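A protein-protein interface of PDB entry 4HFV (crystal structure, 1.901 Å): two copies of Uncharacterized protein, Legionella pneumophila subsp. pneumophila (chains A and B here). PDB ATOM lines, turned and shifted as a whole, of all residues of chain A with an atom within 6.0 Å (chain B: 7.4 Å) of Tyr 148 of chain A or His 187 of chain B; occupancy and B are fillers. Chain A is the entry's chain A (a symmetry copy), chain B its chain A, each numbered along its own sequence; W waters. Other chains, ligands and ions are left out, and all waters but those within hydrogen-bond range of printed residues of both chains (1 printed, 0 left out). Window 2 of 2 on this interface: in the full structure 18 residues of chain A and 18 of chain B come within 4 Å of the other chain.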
ATOM      1  N   VAL A 138     -21.294 -19.663   1.612  1.00  0.00           N
ATOM      2  CA  VAL A 138     -21.464 -19.877   0.185  1.00  0.00           C
ATOM      3  C   VAL A 138     -20.142 -19.659  -0.598  1.00  0.00           C
ATOM      4  O   VAL A 138     -19.804 -20.422  -1.490  1.00  0.00           O
ATOM      5  CB  VAL A 138     -22.569 -18.951  -0.367  1.00  0.00           C
ATOM      6  CG1 VAL A 138     -22.709 -19.112  -1.881  1.00  0.00           C
ATOM      7  CG2 VAL A 138     -23.924 -19.252   0.339  1.00  0.00           C
ATOM      8  N   TYR A 139     -19.409 -18.608  -0.265  1.00  0.00           N
ATOM      9  CA  TYR A 139     -18.201 -18.227  -1.014  1.00  0.00           C
ATOM     10  C   TYR A 139     -16.912 -18.411  -0.219  1.00  0.00           C
ATOM     11  O   TYR A 139     -16.864 -18.189   0.978  1.00  0.00           O
ATOM     12  CB  TYR A 139     -18.295 -16.773  -1.413  1.00  0.00           C
ATOM     13  CG  TYR A 139     -19.588 -16.426  -2.119  1.00  0.00           C
ATOM     14  CD1 TYR A 139     -19.876 -16.950  -3.367  1.00  0.00           C
ATOM     15  CD2 TYR A 139     -20.516 -15.566  -1.534  1.00  0.00           C
ATOM     16  CE1 TYR A 139     -21.026 -16.609  -4.025  1.00  0.00           C
ATOM     17  CE2 TYR A 139     -21.674 -15.238  -2.172  1.00  0.00           C
ATOM     18  CZ  TYR A 139     -21.919 -15.751  -3.423  1.00  0.00           C
ATOM     19  OH  TYR A 139     -23.086 -15.448  -4.050  1.00  0.00           O
ATOM     20  N   LYS A 140     -15.847 -18.782  -0.917  1.00  0.00           N
ATOM     21  CA  LYS A 140     -14.501 -18.728  -0.343  1.00  0.00           C
ATOM     22  C   LYS A 140     -14.236 -17.335   0.220  1.00  0.00           C
ATOM     23  O   LYS A 140     -14.453 -16.333  -0.455  1.00  0.00           O
ATOM     24  CB  LYS A 140     -13.479 -19.116  -1.405  1.00  0.00           C
ATOM     25  CG  LYS A 140     -13.764 -20.527  -1.964  1.00  0.00           C
ATOM     26  CD  LYS A 140     -12.823 -20.904  -3.132  1.00  0.00           C
ATOM     27  CE  LYS A 140     -13.050 -22.354  -3.566  1.00  0.00           C
ATOM     28  NZ  LYS A 140     -12.232 -22.758  -4.738  1.00  0.00           N
ATOM     29  N   PRO A 144     -17.600 -13.327  -3.153  1.00  0.00           N
ATOM     30  CA  PRO A 144     -18.013 -14.020  -4.372  1.00  0.00           C
ATOM     31  C   PRO A 144     -16.958 -13.935  -5.499  1.00  0.00           C
ATOM     32  O   PRO A 144     -16.937 -14.818  -6.367  1.00  0.00           O
ATOM     33  CB  PRO A 144     -19.338 -13.331  -4.738  1.00  0.00           C
ATOM     34  CG  PRO A 144     -19.306 -12.002  -4.000  1.00  0.00           C
ATOM     35  CD  PRO A 144     -18.520 -12.239  -2.768  1.00  0.00           C
ATOM     36  N   LYS A 146     -14.073 -14.724  -5.252  1.00  0.00           N
ATOM     37  CA  LYS A 146     -13.145 -15.838  -5.104  1.00  0.00           C
ATOM     38  C   LYS A 146     -13.834 -17.176  -5.384  1.00  0.00           C
ATOM     39  O   LYS A 146     -13.218 -18.234  -5.244  1.00  0.00           O
ATOM     40  CB  LYS A 146     -12.537 -15.864  -3.694  1.00  0.00           C
ATOM     41  CG  LYS A 146     -11.903 -14.584  -3.207  1.00  0.00           C
ATOM     42  CD  LYS A 146     -10.445 -14.485  -3.638  1.00  0.00           C
ATOM     43  CE  LYS A 146      -9.703 -13.346  -2.905  1.00  0.00           C
ATOM     44  NZ  LYS A 146      -9.772 -13.461  -1.402  1.00  0.00           N
ATOM     45  N   GLY A 147     -15.118 -17.139  -5.738  1.00  0.00           N
ATOM     46  CA  GLY A 147     -15.843 -18.337  -6.095  1.00  0.00           C
ATOM     47  C   GLY A 147     -16.609 -19.011  -4.963  1.00  0.00           C
ATOM     48  O   GLY A 147     -16.579 -18.592  -3.794  1.00  0.00           O
ATOM     49  N   TYR A 148     -17.293 -20.083  -5.335  1.00  0.00           N
ATOM     50  CA  TYR A 148     -18.067 -20.887  -4.401  1.00  0.00           C
ATOM     51  C   TYR A 148     -17.247 -21.923  -3.654  1.00  0.00           C
ATOM     52  O   TYR A 148     -16.356 -22.562  -4.217  1.00  0.00           O
ATOM     53  CB  TYR A 148     -19.146 -21.635  -5.155  1.00  0.00           C
ATOM     54  CG  TYR A 148     -20.315 -20.803  -5.591  1.00  0.00           C
ATOM     55  CD1 TYR A 148     -20.150 -19.729  -6.426  1.00  0.00           C
ATOM     56  CD2 TYR A 148     -21.605 -21.133  -5.189  1.00  0.00           C
ATOM     57  CE1 TYR A 148     -21.238 -18.979  -6.848  1.00  0.00           C
ATOM     58  CE2 TYR A 148     -22.682 -20.417  -5.608  1.00  0.00           C
ATOM     59  CZ  TYR A 148     -22.511 -19.335  -6.414  1.00  0.00           C
ATOM     60  OH  TYR A 148     -23.606 -18.604  -6.814  1.00  0.00           O
ATOM     61  N   LEU A 149     -17.589 -22.109  -2.381  1.00  0.00           N
ATOM     62  CA  LEU A 149     -17.120 -23.264  -1.592  1.00  0.00           C
ATOM     63  C   LEU A 149     -17.534 -24.555  -2.279  1.00  0.00           C
ATOM     64  O   LEU A 149     -18.618 -24.628  -2.833  1.00  0.00           O
ATOM     65  CB  LEU A 149     -17.726 -23.225  -0.180  1.00  0.00           C
ATOM     66  CG  LEU A 149     -17.438 -21.957   0.638  1.00  0.00           C
ATOM     67  CD1 LEU A 149     -18.294 -21.911   1.902  1.00  0.00           C
ATOM     68  CD2 LEU A 149     -15.972 -21.871   0.994  1.00  0.00           C
ATOM     69  N   ASP A 150     -16.673 -25.575  -2.259  1.00  0.00           N
ATOM     70  CA  ASP A 150     -17.011 -26.892  -2.822  1.00  0.00           C
ATOM     71  C   ASP A 150     -18.215 -27.500  -2.079  1.00  0.00           C
ATOM     72  O   ASP A 150     -19.093 -28.122  -2.677  1.00  0.00           O
ATOM     73  CB  ASP A 150     -15.806 -27.870  -2.732  1.00  0.00           C
ATOM     74  CG  ASP A 150     -14.935 -27.871  -3.988  1.00  0.00           C
ATOM     75  OD1 ASP A 150     -15.384 -27.328  -5.027  1.00  0.00           O
ATOM     76  OD2 ASP A 150     -13.804 -28.433  -3.941  1.00  0.00           O
ATOM     77  N   GLN A 152     -21.576 -26.867  -0.113  1.00  0.00           N
ATOM     78  CA  GLN A 152     -22.608 -25.845   0.021  1.00  0.00           C
ATOM     79  C   GLN A 152     -23.663 -26.288   1.050  1.00  0.00           C
ATOM     80  O   GLN A 152     -24.632 -26.949   0.700  1.00  0.00           O
ATOM     81  CB  GLN A 152     -23.265 -25.607  -1.340  1.00  0.00           C
ATOM     82  CG  GLN A 152     -22.370 -24.942  -2.356  1.00  0.00           C
ATOM     83  CD  GLN A 152     -22.175 -23.474  -2.078  1.00  0.00           C
ATOM     84  OE1 GLN A 152     -23.132 -22.746  -1.834  1.00  0.00           O
ATOM     85  NE2 GLN A 152     -20.934 -23.021  -2.145  1.00  0.00           N
ATOM     86  N   VAL A 162     -28.414 -17.777  -2.750  1.00  0.00           N
ATOM     87  CA  VAL A 162     -27.955 -16.538  -3.401  1.00  0.00           C
ATOM     88  C   VAL A 162     -29.084 -15.531  -3.547  1.00  0.00           C
ATOM     89  O   VAL A 162     -28.880 -14.339  -3.328  1.00  0.00           O
ATOM     90  CB  VAL A 162     -27.303 -16.800  -4.787  1.00  0.00           C
ATOM     91  CG1 VAL A 162     -26.923 -15.501  -5.460  1.00  0.00           C
ATOM     92  CG2 VAL A 162     -26.092 -17.664  -4.616  1.00  0.00           C
ATOM     93  N   ILE B 180     -21.968 -10.604  -7.495  1.00  0.00           N
ATOM     94  CA  ILE B 180     -22.695 -11.828  -7.083  1.00  0.00           C
ATOM     95  C   ILE B 180     -23.286 -12.550  -8.275  1.00  0.00           C
ATOM     96  O   ILE B 180     -23.112 -13.768  -8.437  1.00  0.00           O
ATOM     97  CB  ILE B 180     -23.783 -11.484  -6.063  1.00  0.00           C
ATOM     98  CG1 ILE B 180     -23.146 -11.274  -4.689  1.00  0.00           C
ATOM     99  CG2 ILE B 180     -24.819 -12.624  -5.923  1.00  0.00           C
ATOM    100  CD1 ILE B 180     -24.000 -10.438  -3.748  1.00  0.00           C
ATOM    101  N   ILE B 181     -23.975 -11.808  -9.127  1.00  0.00           N
ATOM    102  CA  ILE B 181     -24.597 -12.409 -10.280  1.00  0.00           C
ATOM    103  C   ILE B 181     -23.559 -13.075 -11.203  1.00  0.00           C
ATOM    104  O   ILE B 181     -23.797 -14.142 -11.779  1.00  0.00           O
ATOM    105  CB  ILE B 181     -25.426 -11.372 -11.076  1.00  0.00           C
ATOM    106  CG1 ILE B 181     -26.617 -10.885 -10.235  1.00  0.00           C
ATOM    107  CG2 ILE B 181     -25.892 -11.991 -12.391  1.00  0.00           C
ATOM    108  CD1 ILE B 181     -27.657 -11.927  -9.942  1.00  0.00           C
ATOM    109  N   ALA B 182     -22.408 -12.430 -11.352  1.00  0.00           N
ATOM    110  CA  ALA B 182     -21.400 -12.910 -12.298  1.00  0.00           C
ATOM    111  C   ALA B 182     -20.731 -14.168 -11.750  1.00  0.00           C
ATOM    112  O   ALA B 182     -20.438 -15.088 -12.499  1.00  0.00           O
ATOM    113  CB  ALA B 182     -20.385 -11.829 -12.580  1.00  0.00           C
ATOM    114  N   ALA B 183     -20.555 -14.229 -10.428  1.00  0.00           N
ATOM    115  CA  ALA B 183     -20.011 -15.407  -9.763  1.00  0.00           C
ATOM    116  C   ALA B 183     -20.962 -16.610  -9.877  1.00  0.00           C
ATOM    117  O   ALA B 183     -20.522 -17.751 -10.081  1.00  0.00           O
ATOM    118  CB  ALA B 183     -19.712 -15.096  -8.297  1.00  0.00           C
ATOM    119  N   ARG B 184     -22.263 -16.337  -9.769  1.00  0.00           N
ATOM    120  CA  ARG B 184     -23.297 -17.362  -9.954  1.00  0.00           C
ATOM    121  C   ARG B 184     -23.221 -17.951 -11.366  1.00  0.00           C
ATOM    122  O   ARG B 184     -23.211 -19.172 -11.533  1.00  0.00           O
ATOM    123  CB  ARG B 184     -24.696 -16.778  -9.706  1.00  0.00           C
ATOM    124  CG  ARG B 184     -25.823 -17.846  -9.601  1.00  0.00           C
ATOM    125  CD  ARG B 184     -27.213 -17.225  -9.664  1.00  0.00           C
ATOM    126  NE  ARG B 184     -27.432 -16.544 -10.941  1.00  0.00           N
ATOM    127  CZ  ARG B 184     -28.314 -15.561 -11.145  1.00  0.00           C
ATOM    128  NH1 ARG B 184     -29.085 -15.120 -10.144  1.00  0.00           N
ATOM    129  NH2 ARG B 184     -28.422 -15.005 -12.357  1.00  0.00           N
ATOM    130  N   ASP B 185     -23.153 -17.091 -12.382  1.00  0.00           N
ATOM    131  CA  ASP B 185     -23.106 -17.575 -13.763  1.00  0.00           C
ATOM    132  C   ASP B 185     -21.837 -18.394 -14.002  1.00  0.00           C
ATOM    133  O   ASP B 185     -21.873 -19.403 -14.694  1.00  0.00           O
ATOM    134  CB  ASP B 185     -23.174 -16.421 -14.786  1.00  0.00           C
ATOM    135  CG  ASP B 185     -24.522 -15.691 -14.787  1.00  0.00           C
ATOM    136  OD1 ASP B 185     -24.573 -14.550 -15.309  1.00  0.00           O
ATOM    137  OD2 ASP B 185     -25.522 -16.242 -14.276  1.00  0.00           O
ATOM    138  N   LEU B 186     -20.725 -17.951 -13.426  1.00  0.00           N
ATOM    139  CA  LEU B 186     -19.453 -18.673 -13.526  1.00  0.00           C
ATOM    140  C   LEU B 186     -19.528 -20.043 -12.860  1.00  0.00           C
ATOM    141  O   LEU B 186     -18.959 -21.020 -13.380  1.00  0.00           O
ATOM    142  CB  LEU B 186     -18.307 -17.855 -12.909  1.00  0.00           C
ATOM    143  CG  LEU B 186     -16.866 -18.361 -13.098  1.00  0.00           C
ATOM    144  CD1 LEU B 186     -16.395 -18.223 -14.546  1.00  0.00           C
ATOM    145  CD2 LEU B 186     -15.909 -17.626 -12.167  1.00  0.00           C
ATOM    146  N   HIS B 187     -20.230 -20.100 -11.723  1.00  0.00           N
ATOM    147  CA  HIS B 187     -20.466 -21.330 -10.955  1.00  0.00           C
ATOM    148  C   HIS B 187     -21.294 -22.349 -11.744  1.00  0.00           C
ATOM    149  O   HIS B 187     -20.868 -23.492 -11.981  1.00  0.00           O
ATOM    150  CB  HIS B 187     -21.192 -20.984  -9.636  1.00  0.00           C
ATOM    151  CG  HIS B 187     -21.531 -22.179  -8.793  1.00  0.00           C
ATOM    152  ND1 HIS B 187     -20.594 -23.128  -8.433  1.00  0.00           N
ATOM    153  CD2 HIS B 187     -22.706 -22.589  -8.257  1.00  0.00           C
ATOM    154  CE1 HIS B 187     -21.175 -24.062  -7.703  1.00  0.00           C
ATOM    155  NE2 HIS B 187     -22.457 -23.764  -7.590  1.00  0.00           N
ATOM    156  N   LEU B 188     -22.480 -21.915 -12.157  1.00  0.00           N
ATOM    157  CA  LEU B 188     -23.423 -22.761 -12.883  1.00  0.00           C
ATOM    158  C   LEU B 188     -22.927 -23.145 -14.290  1.00  0.00           C
ATOM    159  O   LEU B 188     -23.347 -24.162 -14.849  1.00  0.00           O
ATOM    160  CB  LEU B 188     -24.770 -22.036 -12.984  1.00  0.00           C
ATOM    161  CG  LEU B 188     -25.373 -21.573 -11.656  1.00  0.00           C
ATOM    162  CD1 LEU B 188     -26.511 -20.585 -11.883  1.00  0.00           C
ATOM    163  CD2 LEU B 188     -25.840 -22.812 -10.861  1.00  0.00           C
ATOM    164  N   LEU B 189     -22.036 -22.328 -14.848  1.00  0.00           N
ATOM    165  CA  LEU B 189     -21.537 -22.509 -16.218  1.00  0.00           C
ATOM    166  C   LEU B 189     -20.052 -22.846 -16.240  1.00  0.00           C
ATOM    167  O   LEU B 189     -19.296 -22.297 -17.046  1.00  0.00           O
ATOM    168  CB  LEU B 189     -21.749 -21.234 -17.045  1.00  0.00           C
ATOM    169  CG  LEU B 189     -23.162 -21.006 -17.568  1.00  0.00           C
ATOM    170  CD1 LEU B 189     -23.461 -19.518 -17.767  1.00  0.00           C
ATOM    171  CD2 LEU B 189     -23.301 -21.796 -18.865  1.00  0.00           C
ATOM    172  N   GLN B 190     -19.628 -23.737 -15.350  1.00  0.00           N
ATOM    173  CA  GLN B 190     -18.229 -24.136 -15.320  1.00  0.00           C
ATOM    174  C   GLN B 190     -18.036 -25.512 -15.965  1.00  0.00           C
ATOM    175  O   GLN B 190     -18.935 -26.029 -16.633  1.00  0.00           O
ATOM    176  CB  GLN B 190     -17.696 -24.118 -13.884  1.00  0.00           C
ATOM    177  CG  GLN B 190     -18.210 -25.223 -12.998  1.00  0.00           C
ATOM    178  CD  GLN B 190     -17.348 -25.384 -11.765  1.00  0.00           C
ATOM    179  OE1 GLN B 190     -17.217 -24.450 -10.959  1.00  0.00           O
ATOM    180  NE2 GLN B 190     -16.728 -26.563 -11.615  1.00  0.00           N
HETATM  181  O   HOH W   1     -23.251 -16.037  -6.695  1.00  0.00           O
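Among the printed residues, merely in contact across the chains: Tyr 148 of chain A with Arg 184 of chain B (3.4 Å), Pro 144 of chain A with Ala 183 of chain B (3.4 Å), Tyr 148 of chain A with His 187 of chain B (3.4 Å), Tyr 148 of chain A with Ala 183 of chain B (3.5 Å), Val 162 of chain A with Ile 180 of chain B (3.6 Å), Tyr 139 of chain A with Ile 180 of chain B (3.8 Å) and Pro 144 of chain A with Ile 180 of chain B (3.97 Å).
Tyr 148 of chain A touches just these residues of chain B: Ala 183 (3.5 Å), Arg 184 (3.4 Å) and His 187 (3.4 Å).
His 187 of chain B touches just one residue of chain A: Tyr 148.
Printed residues of chain A within 4 Å of Ile 180 of chain B: Tyr 139 (3.8 Å), Pro 144 (3.97 Å) and Val 162 (3.6 Å).
Of the printed residues of chain B, Pro 144 of chain A touches Ile 180 (3.97 Å) and Ala 183 (3.4 Å).
Of the printed residues of chain B, Tyr 139 of chain A touches Ile 180 (3.8 Å).
Of the printed residues of chain A, Arg 184 of chain B touches Tyr 148 (3.4 Å).
Printed residues of chain A within 4 Å of Ala 183 of chain B: Pro 144 (3.4 Å) and Tyr 148 (3.5 Å).
Ala 182 of chain B touches none of the printed residues of chain A.
The nearest residue of chain A that does not touch His 187 of chain B is Gln 152 of chain A (5.4 Å).
The nearest printed residue of chain A that does not touch Ile 180 of chain B is Tyr 148 of chain A (5.1 Å).
No position is printed for both chains.
Of the 7 pairs that touch across the chains among the printed residues, none has its exchanged pair printed and touching as well.
Water W1 lies within hydrogen-bond range of OH of Tyr 148 of chain A (2.6 Å), OH of Tyr 139 of chain A (2.7 Å), O of Ile 180 of chain B (2.9 Å) and N of Arg 184 of chain B (3.2 Å).
NH2 of Arg 184 of chain B is in salt-bridge range of OD2 of Asp 185 of chain B.
Along chain A the printed residues that touch a printed residue of chain B span positions 139 to 162.
Printed residues of chain B that touch a printed residue of chain A: Ile 180, Ala 183, Arg 184 and His 187.
Hydrophobic or aromatic side chains of chain B within 4 Å of the printed part of chain A: Ile 180, Ala 183 and His 187.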
